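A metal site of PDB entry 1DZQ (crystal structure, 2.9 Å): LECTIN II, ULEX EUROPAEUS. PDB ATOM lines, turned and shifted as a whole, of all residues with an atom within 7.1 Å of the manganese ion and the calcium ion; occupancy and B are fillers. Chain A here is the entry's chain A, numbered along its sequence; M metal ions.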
ATOM      1  N   ASP A  86     -28.501  21.372  14.349  1.00  0.00           N
ATOM      2  CA  ASP A  86     -28.445  19.978  13.942  1.00  0.00           C
ATOM      3  C   ASP A  86     -27.190  19.264  14.429  1.00  0.00           C
ATOM      4  O   ASP A  86     -27.141  18.023  14.470  1.00  0.00           O
ATOM      5  CB  ASP A  86     -28.459  19.902  12.428  1.00  0.00           C
ATOM      6  CG  ASP A  86     -29.713  19.292  11.909  1.00  0.00           C
ATOM      7  OD1 ASP A  86     -30.696  20.048  11.771  1.00  0.00           O
ATOM      8  OD2 ASP A  86     -29.721  18.070  11.662  1.00  0.00           O
ATOM      9  N   GLY A  87     -26.146  20.042  14.712  1.00  0.00           N
ATOM     10  CA  GLY A  87     -24.892  19.461  15.151  1.00  0.00           C
ATOM     11  C   GLY A  87     -23.677  20.186  14.594  1.00  0.00           C
ATOM     12  O   GLY A  87     -23.797  21.117  13.799  1.00  0.00           O
ATOM     13  N   ALA A 105     -28.545  20.819   6.481  1.00  0.00           N
ATOM     14  CA  ALA A 105     -27.973  20.978   7.813  1.00  0.00           C
ATOM     15  C   ALA A 105     -27.694  19.608   8.436  1.00  0.00           C
ATOM     16  O   ALA A 105     -26.678  19.421   9.119  1.00  0.00           O
ATOM     17  CB  ALA A 105     -28.898  21.768   8.695  1.00  0.00           C
ATOM     18  N   GLY A 106     -28.587  18.657   8.184  1.00  0.00           N
ATOM     19  CA  GLY A 106     -28.419  17.313   8.724  1.00  0.00           C
ATOM     20  C   GLY A 106     -27.189  16.596   8.195  1.00  0.00           C
ATOM     21  O   GLY A 106     -26.784  15.567   8.734  1.00  0.00           O
ATOM     22  N   MET A 107     -26.623  17.130   7.112  1.00  0.00           N
ATOM     23  CA  MET A 107     -25.413  16.565   6.511  1.00  0.00           C
ATOM     24  C   MET A 107     -24.209  17.473   6.761  1.00  0.00           C
ATOM     25  O   MET A 107     -23.120  17.240   6.249  1.00  0.00           O
ATOM     26  CB  MET A 107     -25.643  16.281   5.036  1.00  0.00           C
ATOM     27  CG  MET A 107     -26.783  15.311   4.844  1.00  0.00           C
ATOM     28  SD  MET A 107     -27.106  14.789   3.178  1.00  0.00           S
ATOM     29  CE  MET A 107     -27.919  16.291   2.489  1.00  0.00           C
ATOM     30  N   PHE A 108     -24.434  18.497   7.586  1.00  0.00           N
ATOM     31  CA  PHE A 108     -23.417  19.460   8.005  1.00  0.00           C
ATOM     32  C   PHE A 108     -22.653  20.147   6.886  1.00  0.00           C
ATOM     33  O   PHE A 108     -21.512  20.589   7.087  1.00  0.00           O
ATOM     34  CB  PHE A 108     -22.440  18.780   8.968  1.00  0.00           C
ATOM     35  CG  PHE A 108     -23.111  18.001  10.059  1.00  0.00           C
ATOM     36  CD1 PHE A 108     -23.895  18.632  11.021  1.00  0.00           C
ATOM     37  CD2 PHE A 108     -22.963  16.612  10.134  1.00  0.00           C
ATOM     38  CE1 PHE A 108     -24.528  17.900  12.025  1.00  0.00           C
ATOM     39  CE2 PHE A 108     -23.591  15.873  11.133  1.00  0.00           C
ATOM     40  CZ  PHE A 108     -24.373  16.517  12.078  1.00  0.00           C
ATOM     41  N   GLU A 126     -18.450  13.822  13.893  1.00  0.00           N
ATOM     42  CA  GLU A 126     -19.631  14.613  14.125  1.00  0.00           C
ATOM     43  C   GLU A 126     -20.121  14.584  15.563  1.00  0.00           C
ATOM     44  O   GLU A 126     -19.916  13.609  16.280  1.00  0.00           O
ATOM     45  CB  GLU A 126     -20.761  14.150  13.196  1.00  0.00           C
ATOM     46  CG  GLU A 126     -21.102  12.674  13.327  1.00  0.00           C
ATOM     47  CD  GLU A 126     -22.454  12.317  12.745  1.00  0.00           C
ATOM     48  OE1 GLU A 126     -22.645  12.422  11.514  1.00  0.00           O
ATOM     49  OE2 GLU A 126     -23.349  11.942  13.534  1.00  0.00           O
ATOM     50  N   PHE A 127     -20.740  15.687  15.969  1.00  0.00           N
ATOM     51  CA  PHE A 127     -21.341  15.832  17.292  1.00  0.00           C
ATOM     52  C   PHE A 127     -22.784  16.165  16.914  1.00  0.00           C
ATOM     53  O   PHE A 127     -23.164  17.337  16.806  1.00  0.00           O
ATOM     54  CB  PHE A 127     -20.657  16.955  18.051  1.00  0.00           C
ATOM     55  CG  PHE A 127     -19.197  16.732  18.261  1.00  0.00           C
ATOM     56  CD1 PHE A 127     -18.735  15.975  19.339  1.00  0.00           C
ATOM     57  CD2 PHE A 127     -18.274  17.226  17.353  1.00  0.00           C
ATOM     58  CE1 PHE A 127     -17.380  15.711  19.504  1.00  0.00           C
ATOM     59  CE2 PHE A 127     -16.906  16.964  17.509  1.00  0.00           C
ATOM     60  CZ  PHE A 127     -16.465  16.209  18.586  1.00  0.00           C
ATOM     61  N   ASP A 128     -23.527  15.102  16.613  1.00  0.00           N
ATOM     62  CA  ASP A 128     -24.926  15.117  16.161  1.00  0.00           C
ATOM     63  C   ASP A 128     -25.947  15.338  17.267  1.00  0.00           C
ATOM     64  O   ASP A 128     -26.107  14.501  18.147  1.00  0.00           O
ATOM     65  CB  ASP A 128     -25.196  13.768  15.484  1.00  0.00           C
ATOM     66  CG  ASP A 128     -26.146  13.856  14.325  1.00  0.00           C
ATOM     67  OD1 ASP A 128     -26.976  14.784  14.293  1.00  0.00           O
ATOM     68  OD2 ASP A 128     -26.050  12.974  13.433  1.00  0.00           O
ATOM     69  N   THR A 129     -26.690  16.435  17.188  1.00  0.00           N
ATOM     70  CA  THR A 129     -27.704  16.746  18.199  1.00  0.00           C
ATOM     71  C   THR A 129     -29.121  16.352  17.801  1.00  0.00           C
ATOM     72  O   THR A 129     -30.002  16.244  18.666  1.00  0.00           O
ATOM     73  CB  THR A 129     -27.714  18.238  18.548  1.00  0.00           C
ATOM     74  OG1 THR A 129     -27.847  19.002  17.344  1.00  0.00           O
ATOM     75  CG2 THR A 129     -26.445  18.640  19.262  1.00  0.00           C
ATOM     76  N   TYR A 130     -29.358  16.177  16.505  1.00  0.00           N
ATOM     77  CA  TYR A 130     -30.676  15.791  16.006  1.00  0.00           C
ATOM     78  C   TYR A 130     -30.624  14.370  15.448  1.00  0.00           C
ATOM     79  O   TYR A 130     -29.770  14.057  14.611  1.00  0.00           O
ATOM     80  CB  TYR A 130     -31.157  16.757  14.929  1.00  0.00           C
ATOM     81  CG  TYR A 130     -32.462  16.344  14.294  1.00  0.00           C
ATOM     82  CD1 TYR A 130     -33.676  16.563  14.949  1.00  0.00           C
ATOM     83  CD2 TYR A 130     -32.492  15.712  13.049  1.00  0.00           C
ATOM     84  CE1 TYR A 130     -34.893  16.151  14.377  1.00  0.00           C
ATOM     85  CE2 TYR A 130     -33.697  15.296  12.474  1.00  0.00           C
ATOM     86  CZ  TYR A 130     -34.884  15.517  13.147  1.00  0.00           C
ATOM     87  OH  TYR A 130     -36.082  15.117  12.573  1.00  0.00           O
ATOM     88  N   PHE A 131     -31.589  13.547  15.850  1.00  0.00           N
ATOM     89  CA  PHE A 131     -31.633  12.166  15.404  1.00  0.00           C
ATOM     90  C   PHE A 131     -33.030  11.680  14.997  1.00  0.00           C
ATOM     91  O   PHE A 131     -33.274  10.476  14.933  1.00  0.00           O
ATOM     92  CB  PHE A 131     -31.062  11.260  16.488  1.00  0.00           C
ATOM     93  CG  PHE A 131     -31.744  11.409  17.819  1.00  0.00           C
ATOM     94  CD1 PHE A 131     -31.403  12.451  18.681  1.00  0.00           C
ATOM     95  CD2 PHE A 131     -32.752  10.535  18.200  1.00  0.00           C
ATOM     96  CE1 PHE A 131     -32.048  12.613  19.896  1.00  0.00           C
ATOM     97  CE2 PHE A 131     -33.406  10.688  19.419  1.00  0.00           C
ATOM     98  CZ  PHE A 131     -33.061  11.729  20.268  1.00  0.00           C
ATOM     99  N   GLY A 132     -33.944  12.615  14.728  1.00  0.00           N
ATOM    100  CA  GLY A 132     -35.296  12.247  14.344  1.00  0.00           C
ATOM    101  C   GLY A 132     -35.331  11.306  13.158  1.00  0.00           C
ATOM    102  O   GLY A 132     -34.773  11.607  12.104  1.00  0.00           O
ATOM    103  N   ASN A 136     -33.686  12.116   9.697  1.00  0.00           N
ATOM    104  CA  ASN A 136     -32.343  11.537   9.760  1.00  0.00           C
ATOM    105  C   ASN A 136     -32.438  10.038  10.054  1.00  0.00           C
ATOM    106  O   ASN A 136     -31.986   9.569  11.106  1.00  0.00           O
ATOM    107  CB  ASN A 136     -31.519  12.208  10.877  1.00  0.00           C
ATOM    108  CG  ASN A 136     -31.017  13.593  10.495  1.00  0.00           C
ATOM    109  OD1 ASN A 136     -30.134  14.130  11.159  1.00  0.00           O
ATOM    110  ND2 ASN A 136     -31.571  14.178   9.448  1.00  0.00           N
ATOM    111  N   TRP A 138     -30.719   7.563   9.231  1.00  0.00           N
ATOM    112  CA  TRP A 138     -29.420   6.907   9.420  1.00  0.00           C
ATOM    113  C   TRP A 138     -28.895   6.984  10.862  1.00  0.00           C
ATOM    114  O   TRP A 138     -28.072   6.159  11.262  1.00  0.00           O
ATOM    115  CB  TRP A 138     -28.394   7.528   8.458  1.00  0.00           C
ATOM    116  CG  TRP A 138     -28.330   9.038   8.584  1.00  0.00           C
ATOM    117  CD1 TRP A 138     -27.728   9.765   9.568  1.00  0.00           C
ATOM    118  CD2 TRP A 138     -28.947   9.990   7.714  1.00  0.00           C
ATOM    119  NE1 TRP A 138     -27.944  11.104   9.381  1.00  0.00           N
ATOM    120  CE2 TRP A 138     -28.690  11.266   8.240  1.00  0.00           C
ATOM    121  CE3 TRP A 138     -29.701   9.887   6.536  1.00  0.00           C
ATOM    122  CZ2 TRP A 138     -29.161  12.445   7.635  1.00  0.00           C
ATOM    123  CZ3 TRP A 138     -30.164  11.045   5.929  1.00  0.00           C
ATOM    124  CH2 TRP A 138     -29.892  12.307   6.484  1.00  0.00           C
ATOM    125  N   ASP A 139     -29.338   7.992  11.598  1.00  0.00           N
ATOM    126  CA  ASP A 139     -28.916   8.219  12.983  1.00  0.00           C
ATOM    127  C   ASP A 139     -29.467   7.230  14.006  1.00  0.00           C
ATOM    128  O   ASP A 139     -30.471   6.570  13.760  1.00  0.00           O
ATOM    129  CB  ASP A 139     -29.317   9.630  13.417  1.00  0.00           C
ATOM    130  CG  ASP A 139     -28.318  10.679  12.944  1.00  0.00           C
ATOM    131  OD1 ASP A 139     -27.084  10.405  12.868  1.00  0.00           O
ATOM    132  OD2 ASP A 139     -28.796  11.735  12.588  1.00  0.00           O
ATOM    133  N   PRO A 140     -28.712   6.982  15.104  1.00  0.00           N
ATOM    134  CA  PRO A 140     -29.158   6.104  16.204  1.00  0.00           C
ATOM    135  C   PRO A 140     -30.181   6.877  17.035  1.00  0.00           C
ATOM    136  O   PRO A 140     -30.423   8.054  16.752  1.00  0.00           O
ATOM    137  CB  PRO A 140     -27.870   5.828  16.975  1.00  0.00           C
ATOM    138  CG  PRO A 140     -27.077   7.058  16.744  1.00  0.00           C
ATOM    139  CD  PRO A 140     -27.279   7.292  15.280  1.00  0.00           C
ATOM    140  N   PHE A 142     -30.288   8.606  19.822  1.00  0.00           N
ATOM    141  CA  PHE A 142     -29.751   9.501  20.844  1.00  0.00           C
ATOM    142  C   PHE A 142     -28.741  10.461  20.261  1.00  0.00           C
ATOM    143  O   PHE A 142     -28.239  10.252  19.147  1.00  0.00           O
ATOM    144  CB  PHE A 142     -29.102   8.688  21.974  1.00  0.00           C
ATOM    145  CG  PHE A 142     -28.207   7.571  21.484  1.00  0.00           C
ATOM    146  CD1 PHE A 142     -26.916   7.842  21.004  1.00  0.00           C
ATOM    147  CD2 PHE A 142     -28.655   6.253  21.472  1.00  0.00           C
ATOM    148  CE1 PHE A 142     -26.099   6.820  20.530  1.00  0.00           C
ATOM    149  CE2 PHE A 142     -27.839   5.224  21.007  1.00  0.00           C
ATOM    150  CZ  PHE A 142     -26.565   5.513  20.526  1.00  0.00           C
ATOM    151  N   HIS A 144     -25.354  11.795  19.530  1.00  0.00           N
ATOM    152  CA  HIS A 144     -24.140  11.001  19.455  1.00  0.00           C
ATOM    153  C   HIS A 144     -22.893  11.684  18.905  1.00  0.00           C
ATOM    154  O   HIS A 144     -22.925  12.826  18.461  1.00  0.00           O
ATOM    155  CB  HIS A 144     -24.431   9.783  18.571  1.00  0.00           C
ATOM    156  CG  HIS A 144     -25.041  10.147  17.247  1.00  0.00           C
ATOM    157  ND1 HIS A 144     -26.361  10.519  17.109  1.00  0.00           N
ATOM    158  CD2 HIS A 144     -24.485  10.263  16.016  1.00  0.00           C
ATOM    159  CE1 HIS A 144     -26.590  10.854  15.854  1.00  0.00           C
ATOM    160  NE2 HIS A 144     -25.468  10.711  15.174  1.00  0.00           N
ATOM    161  N   ILE A 145     -21.784  10.948  18.982  1.00  0.00           N
ATOM    162  CA  ILE A 145     -20.506  11.362  18.449  1.00  0.00           C
ATOM    163  C   ILE A 145     -20.279  10.262  17.433  1.00  0.00           C
ATOM    164  O   ILE A 145     -20.363   9.082  17.769  1.00  0.00           O
ATOM    165  CB  ILE A 145     -19.372  11.277  19.488  1.00  0.00           C
ATOM    166  CG1 ILE A 145     -19.598  12.277  20.617  1.00  0.00           C
ATOM    167  CG2 ILE A 145     -18.024  11.528  18.803  1.00  0.00           C
ATOM    168  CD1 ILE A 145     -18.516  12.228  21.680  1.00  0.00           C
ATOM    169  N   GLY A 146     -20.021  10.627  16.179  1.00  0.00           N
ATOM    170  CA  GLY A 146     -19.820   9.598  15.178  1.00  0.00           C
ATOM    171  C   GLY A 146     -18.635   9.833  14.282  1.00  0.00           C
ATOM    172  O   GLY A 146     -18.283  10.977  13.998  1.00  0.00           O
ATOM    173  N   ASP A 148     -17.456   9.573  10.739  1.00  0.00           N
ATOM    174  CA  ASP A 148     -18.019   9.460   9.406  1.00  0.00           C
ATOM    175  C   ASP A 148     -16.935   9.273   8.374  1.00  0.00           C
ATOM    176  O   ASP A 148     -15.952  10.024   8.356  1.00  0.00           O
ATOM    177  CB  ASP A 148     -18.827  10.708   9.041  1.00  0.00           C
ATOM    178  CG  ASP A 148     -19.983  10.951   9.981  1.00  0.00           C
ATOM    179  OD1 ASP A 148     -20.269  10.104  10.852  1.00  0.00           O
ATOM    180  OD2 ASP A 148     -20.614  12.016   9.863  1.00  0.00           O
ATOM    181  N   ILE A 152     -22.767  10.149   5.667  1.00  0.00           N
ATOM    182  CA  ILE A 152     -23.378  10.755   6.847  1.00  0.00           C
ATOM    183  C   ILE A 152     -23.823   9.668   7.842  1.00  0.00           C
ATOM    184  O   ILE A 152     -24.185   9.961   8.987  1.00  0.00           O
ATOM    185  CB  ILE A 152     -24.557  11.681   6.464  1.00  0.00           C
ATOM    186  CG1 ILE A 152     -24.977  12.549   7.658  1.00  0.00           C
ATOM    187  CG2 ILE A 152     -25.724  10.869   5.932  1.00  0.00           C
ATOM    188  CD1 ILE A 152     -23.889  13.483   8.151  1.00  0.00           C
ATOM    189  N   LYS A 153     -23.833   8.424   7.369  1.00  0.00           N
ATOM    190  CA  LYS A 153     -24.186   7.273   8.191  1.00  0.00           C
ATOM    191  C   LYS A 153     -22.848   6.817   8.781  1.00  0.00           C
ATOM    192  O   LYS A 153     -22.036   6.172   8.097  1.00  0.00           O
ATOM    193  CB  LYS A 153     -24.824   6.176   7.342  1.00  0.00           C
ATOM    194  CG  LYS A 153     -25.168   4.895   8.124  1.00  0.00           C
ATOM    195  CD  LYS A 153     -25.955   3.893   7.273  1.00  0.00           C
ATOM    196  CE  LYS A 153     -26.019   2.520   7.932  1.00  0.00           C
ATOM    197  NZ  LYS A 153     -26.589   2.572   9.312  1.00  0.00           N
ATOM    198  N   SER A 154     -22.605   7.234  10.016  1.00  0.00           N
ATOM    199  CA  SER A 154     -21.385   6.952  10.761  1.00  0.00           C
ATOM    200  C   SER A 154     -21.063   5.467  10.802  1.00  0.00           C
ATOM    201  O   SER A 154     -21.961   4.639  10.896  1.00  0.00           O
ATOM    202  CB  SER A 154     -21.509   7.487  12.183  1.00  0.00           C
ATOM    203  OG  SER A 154     -22.209   8.733  12.229  1.00  0.00           O
ATOM    204  N   THR A 157     -20.607   4.943  16.306  1.00  0.00           N
ATOM    205  CA  THR A 157     -21.096   6.043  17.124  1.00  0.00           C
ATOM    206  C   THR A 157     -21.030   5.691  18.606  1.00  0.00           C
ATOM    207  O   THR A 157     -20.739   4.547  18.974  1.00  0.00           O
ATOM    208  CB  THR A 157     -22.560   6.422  16.795  1.00  0.00           C
ATOM    209  OG1 THR A 157     -23.413   5.314  17.093  1.00  0.00           O
ATOM    210  CG2 THR A 157     -22.701   6.788  15.329  1.00  0.00           C
HETATM  211 MN    MN M   1     -25.205  11.126  13.054  1.00  0.00          MN
HETATM  212 CA    CA M   2     -28.330  14.240  12.573  1.00  0.00          CA
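The side-chain carboxylate (OD2) of Asp 139 lies close to the indole nitrogen (NE1) of Trp 138 (3.4 Å). The side-chain carboxylate of Glu 126 lies close to the side-chain carboxylate of Asp 148 (2.6 Å). O of Gly 146 is in hydrogen-bond range of N of Glu 126, 2.9 Å away. The backbone carbonyl oxygen (O) of Phe 142 lies within hydrogen-bond range of a ring nitrogen (ND1) of His 144 (2.8 Å). The side-chain hydroxyl (OG) of Ser 154 lies within hydrogen-bond range of the side-chain carboxylate (OD1) of Asp 148 (2.7 Å).
Residues that only touch the manganese ion: Ser 154 (3.9 Å). Within 4 Å of the manganese ion: Glu 126, Asp 128, Asp 139, His 144 and Ser 154. The nearest printed residue that does not touch the manganese ion is Ile 152 (4.4 Å).
The nearest printed residue that does not touch the calcium ion is Asp 86 (4.2 Å).
The manganese ion is bound by OD1 of Asp 139 (2.0 Å), OD2 of Asp 128 (2.1 Å), OE2 of Glu 126 (2.1 Å) and NE2 of His 144 (2.2 Å).
OD1 of Asp 128 binds the calcium ion, at 2.3 Å. The calcium ion is bound by the side-chain amide oxygen (OD1) of Asn 136, 2.3 Å away. O of Tyr 130 is bound to the calcium ion, 2.5 Å away. The calcium ion is bound by the side-chain carboxylate (OD2) of Asp 139, 2.5 Å away. OD2 of Asp 128 binds the calcium ion (2.7 Å). The calcium ion has five donor atoms within binding distance.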
